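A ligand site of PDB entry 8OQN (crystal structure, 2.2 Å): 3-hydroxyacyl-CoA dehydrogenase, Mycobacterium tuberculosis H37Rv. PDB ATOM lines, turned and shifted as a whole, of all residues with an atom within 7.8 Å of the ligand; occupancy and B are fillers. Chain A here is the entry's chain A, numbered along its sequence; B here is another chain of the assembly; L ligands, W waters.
The backbone NH of Gln 310 lies within hydrogen-bond range of an oxygen (O2) of the ligand (2.9 Å).
The backbone NH of Val 311 sits at hydrogen-bond distance from an oxygen (O2) of the ligand (3.2 Å).
Pro 273 touches the ligand (C to C4, 3.4 Å).
Met 274 touches the ligand.
Pro 275 touches the ligand (N to C4, 3.6 Å).
CD of Arg 278 touches C5 of the ligand, at 3.6 Å.
CA of Gly 309 touches O2 of the ligand (3.5 Å).
Tyr 142 of chain B touches the ligand.
Hydrophobic or aromatic side chains within 4 Å of the ligand: Pro 275, Val 311 and Tyr 142 of chain B.
Within 4 Å of the ligand: Pro 273, Met 274, Pro 275, Arg 278, Gly 309, Gln 310, Val 311 and Tyr 142 of chain B.
Water W1 lies within hydrogen-bond range of O of Leu 306 (2.8 Å), N of Ala 312 (2.9 Å) and O2 of the ligand (3.2 Å).
The side-chain amide oxygen of Asn 314 lies within hydrogen-bond range of the side-chain amide nitrogen of Gln 310 (2.8 Å).
The side-chain carboxylate of Asp 143 of chain B lies within salt-bridge range of the guanidinium group of Arg 278 (3.0 Å).
NH1 of Arg 266 lies within hydrogen-bond range of O of Tyr 142 of chain B (2.8 Å).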
ATOM      1  N   GLY A 161     -19.088   4.375  -1.462  1.00  0.00           N
ATOM      2  CA  GLY A 161     -18.439   3.710  -2.572  1.00  0.00           C
ATOM      3  C   GLY A 161     -17.623   2.502  -2.182  1.00  0.00           C
ATOM      4  O   GLY A 161     -16.733   2.096  -2.934  1.00  0.00           O
ATOM      5  N   ARG A 266     -28.792  -3.153 -13.200  1.00  0.00           N
ATOM      6  CA  ARG A 266     -28.608  -2.110 -14.212  1.00  0.00           C
ATOM      7  C   ARG A 266     -29.860  -1.245 -14.339  1.00  0.00           C
ATOM      8  O   ARG A 266     -29.764  -0.037 -14.570  1.00  0.00           O
ATOM      9  CB  ARG A 266     -28.246  -2.728 -15.563  1.00  0.00           C
ATOM     10  CG  ARG A 266     -26.861  -3.324 -15.631  1.00  0.00           C
ATOM     11  CD  ARG A 266     -26.434  -3.545 -17.082  1.00  0.00           C
ATOM     12  NE  ARG A 266     -26.028  -2.310 -17.734  1.00  0.00           N
ATOM     13  CZ  ARG A 266     -24.767  -1.915 -17.868  1.00  0.00           C
ATOM     14  NH1 ARG A 266     -23.759  -2.648 -17.412  1.00  0.00           N
ATOM     15  NH2 ARG A 266     -24.510  -0.764 -18.491  1.00  0.00           N
ATOM     16  N   LEU A 269     -29.817   1.153 -11.270  1.00  0.00           N
ATOM     17  CA  LEU A 269     -28.759   2.148 -11.401  1.00  0.00           C
ATOM     18  C   LEU A 269     -28.847   2.922 -12.707  1.00  0.00           C
ATOM     19  O   LEU A 269     -28.120   3.911 -12.871  1.00  0.00           O
ATOM     20  CB  LEU A 269     -27.383   1.484 -11.286  1.00  0.00           C
ATOM     21  CG  LEU A 269     -27.056   0.848  -9.934  1.00  0.00           C
ATOM     22  CD1 LEU A 269     -25.624   0.336  -9.919  1.00  0.00           C
ATOM     23  CD2 LEU A 269     -27.284   1.851  -8.805  1.00  0.00           C
ATOM     24  N   GLY A 271     -27.694   2.386 -15.533  1.00  0.00           N
ATOM     25  CA  GLY A 271     -26.451   2.425 -16.262  1.00  0.00           C
ATOM     26  C   GLY A 271     -25.412   3.388 -15.739  1.00  0.00           C
ATOM     27  O   GLY A 271     -24.381   3.590 -16.400  1.00  0.00           O
ATOM     28  N   ALA A 272     -25.647   4.008 -14.580  1.00  0.00           N
ATOM     29  CA  ALA A 272     -24.701   4.968 -14.043  1.00  0.00           C
ATOM     30  C   ALA A 272     -23.402   4.270 -13.637  1.00  0.00           C
ATOM     31  O   ALA A 272     -23.408   3.099 -13.260  1.00  0.00           O
ATOM     32  CB  ALA A 272     -25.307   5.686 -12.840  1.00  0.00           C
ATOM     33  N   PRO A 273     -22.271   4.977 -13.727  1.00  0.00           N
ATOM     34  CA  PRO A 273     -20.970   4.339 -13.414  1.00  0.00           C
ATOM     35  C   PRO A 273     -20.645   4.318 -11.929  1.00  0.00           C
ATOM     36  O   PRO A 273     -19.718   4.979 -11.442  1.00  0.00           O
ATOM     37  CB  PRO A 273     -19.995   5.197 -14.231  1.00  0.00           C
ATOM     38  CG  PRO A 273     -20.607   6.563 -14.189  1.00  0.00           C
ATOM     39  CD  PRO A 273     -22.101   6.342 -14.245  1.00  0.00           C
ATOM     40  N   MET A 274     -21.409   3.542 -11.164  1.00  0.00           N
ATOM     41  CA  MET A 274     -21.163   3.360  -9.744  1.00  0.00           C
ATOM     42  C   MET A 274     -20.733   1.922  -9.497  1.00  0.00           C
ATOM     43  O   MET A 274     -21.578   1.009  -9.521  1.00  0.00           O
ATOM     44  CB  MET A 274     -22.401   3.711  -8.919  1.00  0.00           C
ATOM     45  CG  MET A 274     -22.083   4.400  -7.607  1.00  0.00           C
ATOM     46  SD  MET A 274     -23.529   5.061  -6.751  1.00  0.00           S
ATOM     47  CE  MET A 274     -24.332   3.557  -6.223  1.00  0.00           C
ATOM     48  N   PRO A 275     -19.451   1.654  -9.240  1.00  0.00           N
ATOM     49  CA  PRO A 275     -18.955   0.271  -9.257  1.00  0.00           C
ATOM     50  C   PRO A 275     -19.247  -0.528  -7.990  1.00  0.00           C
ATOM     51  O   PRO A 275     -19.171  -1.764  -8.040  1.00  0.00           O
ATOM     52  CB  PRO A 275     -17.444   0.432  -9.457  1.00  0.00           C
ATOM     53  CG  PRO A 275     -17.140   1.751  -8.823  1.00  0.00           C
ATOM     54  CD  PRO A 275     -18.338   2.629  -9.093  1.00  0.00           C
ATOM     55  N   ALA A 276     -19.559   0.123  -6.866  1.00  0.00           N
ATOM     56  CA  ALA A 276     -19.708  -0.613  -5.609  1.00  0.00           C
ATOM     57  C   ALA A 276     -20.853  -1.614  -5.634  1.00  0.00           C
ATOM     58  O   ALA A 276     -20.636  -2.765  -5.219  1.00  0.00           O
ATOM     59  CB  ALA A 276     -19.849   0.378  -4.450  1.00  0.00           C
ATOM     60  N   PRO A 277     -22.078  -1.268  -6.069  1.00  0.00           N
ATOM     61  CA  PRO A 277     -23.128  -2.299  -6.108  1.00  0.00           C
ATOM     62  C   PRO A 277     -22.776  -3.491  -6.972  1.00  0.00           C
ATOM     63  O   PRO A 277     -23.087  -4.633  -6.615  1.00  0.00           O
ATOM     64  CB  PRO A 277     -24.342  -1.531  -6.663  1.00  0.00           C
ATOM     65  CG  PRO A 277     -24.087  -0.122  -6.305  1.00  0.00           C
ATOM     66  CD  PRO A 277     -22.604   0.050  -6.452  1.00  0.00           C
ATOM     67  N   ARG A 278     -22.137  -3.254  -8.123  1.00  0.00           N
ATOM     68  CA  ARG A 278     -21.705  -4.351  -8.977  1.00  0.00           C
ATOM     69  C   ARG A 278     -20.713  -5.262  -8.259  1.00  0.00           C
ATOM     70  O   ARG A 278     -20.778  -6.491  -8.370  1.00  0.00           O
ATOM     71  CB  ARG A 278     -21.082  -3.799 -10.251  1.00  0.00           C
ATOM     72  CG  ARG A 278     -20.322  -4.806 -11.088  1.00  0.00           C
ATOM     73  CD  ARG A 278     -19.398  -4.094 -12.069  1.00  0.00           C
ATOM     74  NE  ARG A 278     -18.598  -5.031 -12.861  1.00  0.00           N
ATOM     75  CZ  ARG A 278     -17.470  -5.590 -12.443  1.00  0.00           C
ATOM     76  NH1 ARG A 278     -16.994  -5.369 -11.235  1.00  0.00           N
ATOM     77  NH2 ARG A 278     -16.813  -6.399 -13.276  1.00  0.00           N
ATOM     78  N   ALA A 279     -19.779  -4.672  -7.498  1.00  0.00           N
ATOM     79  CA  ALA A 279     -18.794  -5.468  -6.775  1.00  0.00           C
ATOM     80  C   ALA A 279     -19.453  -6.264  -5.656  1.00  0.00           C
ATOM     81  O   ALA A 279     -19.033  -7.385  -5.365  1.00  0.00           O
ATOM     82  CB  ALA A 279     -17.692  -4.564  -6.226  1.00  0.00           C
ATOM     83  N   ALA A 304     -10.628  -4.281  -1.847  1.00  0.00           N
ATOM     84  CA  ALA A 304      -9.468  -3.496  -2.248  1.00  0.00           C
ATOM     85  C   ALA A 304      -9.662  -2.867  -3.625  1.00  0.00           C
ATOM     86  O   ALA A 304      -9.087  -1.812  -3.905  1.00  0.00           O
ATOM     87  CB  ALA A 304      -8.216  -4.379  -2.249  1.00  0.00           C
ATOM     88  N   SER A 305     -10.465  -3.496  -4.482  1.00  0.00           N
ATOM     89  CA  SER A 305     -10.720  -2.941  -5.812  1.00  0.00           C
ATOM     90  C   SER A 305     -11.485  -1.630  -5.720  1.00  0.00           C
ATOM     91  O   SER A 305     -11.234  -0.708  -6.503  1.00  0.00           O
ATOM     92  CB  SER A 305     -11.493  -3.959  -6.663  1.00  0.00           C
ATOM     93  OG  SER A 305     -11.765  -3.446  -7.945  1.00  0.00           O
ATOM     94  N   LEU A 306     -12.411  -1.525  -4.772  1.00  0.00           N
ATOM     95  CA  LEU A 306     -13.175  -0.292  -4.619  1.00  0.00           C
ATOM     96  C   LEU A 306     -12.374   0.773  -3.892  1.00  0.00           C
ATOM     97  O   LEU A 306     -12.412   1.954  -4.272  1.00  0.00           O
ATOM     98  CB  LEU A 306     -14.475  -0.578  -3.871  1.00  0.00           C
ATOM     99  CG  LEU A 306     -15.484  -1.498  -4.563  1.00  0.00           C
ATOM    100  CD1 LEU A 306     -16.654  -1.798  -3.657  1.00  0.00           C
ATOM    101  CD2 LEU A 306     -15.956  -0.878  -5.861  1.00  0.00           C
ATOM    102  N   VAL A 307     -11.639   0.389  -2.840  1.00  0.00           N
ATOM    103  CA  VAL A 307     -10.945   1.363  -1.999  1.00  0.00           C
ATOM    104  C   VAL A 307      -9.909   2.134  -2.800  1.00  0.00           C
ATOM    105  O   VAL A 307      -9.766   3.352  -2.643  1.00  0.00           O
ATOM    106  CB  VAL A 307     -10.312   0.654  -0.789  1.00  0.00           C
ATOM    107  CG1 VAL A 307      -9.316   1.565  -0.081  1.00  0.00           C
ATOM    108  CG2 VAL A 307     -11.395   0.195   0.174  1.00  0.00           C
ATOM    109  N   THR A 308      -9.183   1.449  -3.688  1.00  0.00           N
ATOM    110  CA  THR A 308      -8.145   2.107  -4.485  1.00  0.00           C
ATOM    111  C   THR A 308      -8.694   2.789  -5.726  1.00  0.00           C
ATOM    112  O   THR A 308      -7.909   3.404  -6.462  1.00  0.00           O
ATOM    113  CB  THR A 308      -7.077   1.090  -4.882  1.00  0.00           C
ATOM    114  OG1 THR A 308      -7.677  -0.001  -5.594  1.00  0.00           O
ATOM    115  CG2 THR A 308      -6.369   0.537  -3.644  1.00  0.00           C
ATOM    116  N   GLY A 309     -10.005   2.713  -5.979  1.00  0.00           N
ATOM    117  CA  GLY A 309     -10.597   3.355  -7.128  1.00  0.00           C
ATOM    118  C   GLY A 309     -10.953   4.816  -6.866  1.00  0.00           C
ATOM    119  O   GLY A 309     -10.902   5.305  -5.744  1.00  0.00           O
ATOM    120  N   GLN A 310     -11.345   5.509  -7.944  1.00  0.00           N
ATOM    121  CA  GLN A 310     -11.582   6.941  -7.855  1.00  0.00           C
ATOM    122  C   GLN A 310     -12.975   7.274  -7.319  1.00  0.00           C
ATOM    123  O   GLN A 310     -13.138   8.265  -6.604  1.00  0.00           O
ATOM    124  CB  GLN A 310     -11.389   7.597  -9.224  1.00  0.00           C
ATOM    125  CG  GLN A 310     -11.539   9.110  -9.202  1.00  0.00           C
ATOM    126  CD  GLN A 310     -10.644   9.784  -8.176  1.00  0.00           C
ATOM    127  OE1 GLN A 310      -9.453   9.471  -8.088  1.00  0.00           O
ATOM    128  NE2 GLN A 310     -11.207  10.691  -7.394  1.00  0.00           N
ATOM    129  N   VAL A 311     -13.985   6.460  -7.642  1.00  0.00           N
ATOM    130  CA  VAL A 311     -15.355   6.758  -7.219  1.00  0.00           C
ATOM    131  C   VAL A 311     -15.452   6.734  -5.694  1.00  0.00           C
ATOM    132  O   VAL A 311     -16.126   7.581  -5.093  1.00  0.00           O
ATOM    133  CB  VAL A 311     -16.355   5.791  -7.869  1.00  0.00           C
ATOM    134  CG1 VAL A 311     -17.731   5.925  -7.237  1.00  0.00           C
ATOM    135  CG2 VAL A 311     -16.442   6.048  -9.359  1.00  0.00           C
ATOM    136  N   ALA A 312     -14.789   5.770  -5.053  1.00  0.00           N
ATOM    137  CA  ALA A 312     -14.806   5.714  -3.595  1.00  0.00           C
ATOM    138  C   ALA A 312     -14.175   6.952  -2.985  1.00  0.00           C
ATOM    139  O   ALA A 312     -14.619   7.445  -1.936  1.00  0.00           O
ATOM    140  CB  ALA A 312     -14.099   4.457  -3.107  1.00  0.00           C
ATOM    141  N   LYS A 313     -13.136   7.492  -3.639  1.00  0.00           N
ATOM    142  CA  LYS A 313     -12.492   8.696  -3.125  1.00  0.00           C
ATOM    143  C   LYS A 313     -13.409   9.913  -3.284  1.00  0.00           C
ATOM    144  O   LYS A 313     -13.427  10.794  -2.421  1.00  0.00           O
ATOM    145  CB  LYS A 313     -11.155   8.917  -3.825  1.00  0.00           C
ATOM    146  CG  LYS A 313     -10.179   7.774  -3.610  1.00  0.00           C
ATOM    147  CD  LYS A 313      -8.906   7.948  -4.406  1.00  0.00           C
ATOM    148  CE  LYS A 313      -8.082   6.670  -4.359  1.00  0.00           C
ATOM    149  NZ  LYS A 313      -7.996   6.137  -2.979  1.00  0.00           N
ATOM    150  N   ASN A 314     -14.166   9.967  -4.375  1.00  0.00           N
ATOM    151  CA  ASN A 314     -15.167  11.017  -4.533  1.00  0.00           C
ATOM    152  C   ASN A 314     -16.200  10.942  -3.411  1.00  0.00           C
ATOM    153  O   ASN A 314     -16.502  11.949  -2.756  1.00  0.00           O
ATOM    154  CB  ASN A 314     -15.856  10.909  -5.893  1.00  0.00           C
ATOM    155  CG  ASN A 314     -14.888  11.032  -7.044  1.00  0.00           C
ATOM    156  OD1 ASN A 314     -13.805  11.592  -6.903  1.00  0.00           O
ATOM    157  ND2 ASN A 314     -15.278  10.498  -8.204  1.00  0.00           N
ATOM    158  N   TRP A 691     -21.812   9.627  -7.376  1.00  0.00           N
ATOM    159  CA  TRP A 691     -20.531   9.006  -7.680  1.00  0.00           C
ATOM    160  C   TRP A 691     -19.450  10.036  -7.995  1.00  0.00           C
ATOM    161  O   TRP A 691     -18.260   9.737  -7.838  1.00  0.00           O
ATOM    162  CB  TRP A 691     -20.673   8.027  -8.843  1.00  0.00           C
ATOM    163  CG  TRP A 691     -20.936   8.667 -10.181  1.00  0.00           C
ATOM    164  CD1 TRP A 691     -22.162   8.864 -10.764  1.00  0.00           C
ATOM    165  CD2 TRP A 691     -19.970   9.168 -11.109  1.00  0.00           C
ATOM    166  NE1 TRP A 691     -22.010   9.463 -11.992  1.00  0.00           N
ATOM    167  CE2 TRP A 691     -20.671   9.666 -12.226  1.00  0.00           C
ATOM    168  CE3 TRP A 691     -18.574   9.251 -11.096  1.00  0.00           C
ATOM    169  CZ2 TRP A 691     -20.025  10.234 -13.311  1.00  0.00           C
ATOM    170  CZ3 TRP A 691     -17.928   9.819 -12.181  1.00  0.00           C
ATOM    171  CH2 TRP A 691     -18.656  10.299 -13.279  1.00  0.00           C
ATOM    172  N   SER A 703     -12.136  11.407 -14.471  1.00  0.00           N
ATOM    173  CA  SER A 703     -11.387  10.293 -15.043  1.00  0.00           C
ATOM    174  C   SER A 703     -11.954   9.985 -16.419  1.00  0.00           C
ATOM    175  O   SER A 703     -13.148   9.727 -16.552  1.00  0.00           O
ATOM    176  CB  SER A 703     -11.450   9.060 -14.140  1.00  0.00           C
ATOM    177  OG  SER A 703     -10.702   7.986 -14.691  1.00  0.00           O
ATOM    178  N   ALA B 139     -20.324 -10.333 -12.466  1.00  0.00           N
ATOM    179  CA  ALA B 139     -19.373  -9.383 -13.020  1.00  0.00           C
ATOM    180  C   ALA B 139     -19.334  -9.469 -14.542  1.00  0.00           C
ATOM    181  O   ALA B 139     -19.349  -8.437 -15.230  1.00  0.00           O
ATOM    182  CB  ALA B 139     -17.981  -9.617 -12.430  1.00  0.00           C
ATOM    183  N   TYR B 142     -22.841  -8.413 -15.981  1.00  0.00           N
ATOM    184  CA  TYR B 142     -23.025  -6.972 -15.895  1.00  0.00           C
ATOM    185  C   TYR B 142     -22.263  -6.242 -16.998  1.00  0.00           C
ATOM    186  O   TYR B 142     -22.743  -5.228 -17.519  1.00  0.00           O
ATOM    187  CB  TYR B 142     -22.565  -6.486 -14.517  1.00  0.00           C
ATOM    188  CG  TYR B 142     -22.955  -5.080 -14.146  1.00  0.00           C
ATOM    189  CD1 TYR B 142     -22.158  -4.004 -14.504  1.00  0.00           C
ATOM    190  CD2 TYR B 142     -24.112  -4.829 -13.422  1.00  0.00           C
ATOM    191  CE1 TYR B 142     -22.507  -2.708 -14.153  1.00  0.00           C
ATOM    192  CE2 TYR B 142     -24.469  -3.542 -13.063  1.00  0.00           C
ATOM    193  CZ  TYR B 142     -23.667  -2.486 -13.440  1.00  0.00           C
ATOM    194  OH  TYR B 142     -24.018  -1.200 -13.090  1.00  0.00           O
ATOM    195  N   ASP B 143     -21.092  -6.759 -17.370  1.00  0.00           N
ATOM    196  CA  ASP B 143     -20.240  -6.034 -18.326  1.00  0.00           C
ATOM    197  C   ASP B 143     -20.640  -6.311 -19.766  1.00  0.00           C
ATOM    198  O   ASP B 143     -20.668  -5.395 -20.587  1.00  0.00           O
ATOM    199  CB  ASP B 143     -18.781  -6.401 -18.088  1.00  0.00           C
ATOM    200  CG  ASP B 143     -18.279  -5.943 -16.732  1.00  0.00           C
ATOM    201  OD1 ASP B 143     -18.812  -4.943 -16.214  1.00  0.00           O
ATOM    202  OD2 ASP B 143     -17.349  -6.585 -16.185  1.00  0.00           O
HETATM  203  N1  LIG L   1     -15.349   3.070 -12.913  1.00  0.00           N
HETATM  204  C1  LIG L   1     -14.661   1.373 -11.621  1.00  0.00           C
HETATM  205  C2  LIG L   1     -14.314   2.546 -10.969  1.00  0.00           C
HETATM  206  C3  LIG L   1     -14.772   3.560 -11.827  1.00  0.00           C
HETATM  207  O1  LIG L   1     -13.296   1.568  -9.069  1.00  0.00           O
HETATM  208  C4  LIG L   1     -19.483   1.304 -12.822  1.00  0.00           C
HETATM  209  C5  LIG L   1     -19.202  -0.903 -13.667  1.00  0.00           C
HETATM  210  C6  LIG L   1     -15.841   0.851 -13.798  1.00  0.00           C
HETATM  211  C7  LIG L   1     -17.858  -0.651 -13.887  1.00  0.00           C
HETATM  212  C8  LIG L   1     -17.313   0.586 -13.572  1.00  0.00           C
HETATM  213  C9  LIG L   1     -18.138   1.556 -13.042  1.00  0.00           C
HETATM  214  C10 LIG L   1     -13.610   2.687  -9.658  1.00  0.00           C
HETATM  215  O2  LIG L   1     -13.363   3.788  -9.191  1.00  0.00           O
HETATM  216  N2  LIG L   1     -15.269   1.729 -12.760  1.00  0.00           N
HETATM  217  C11 LIG L   1     -20.012   0.075 -13.139  1.00  0.00           C
HETATM  218  O   HOH W   1     -14.008   3.161  -6.160  1.00  0.00           O
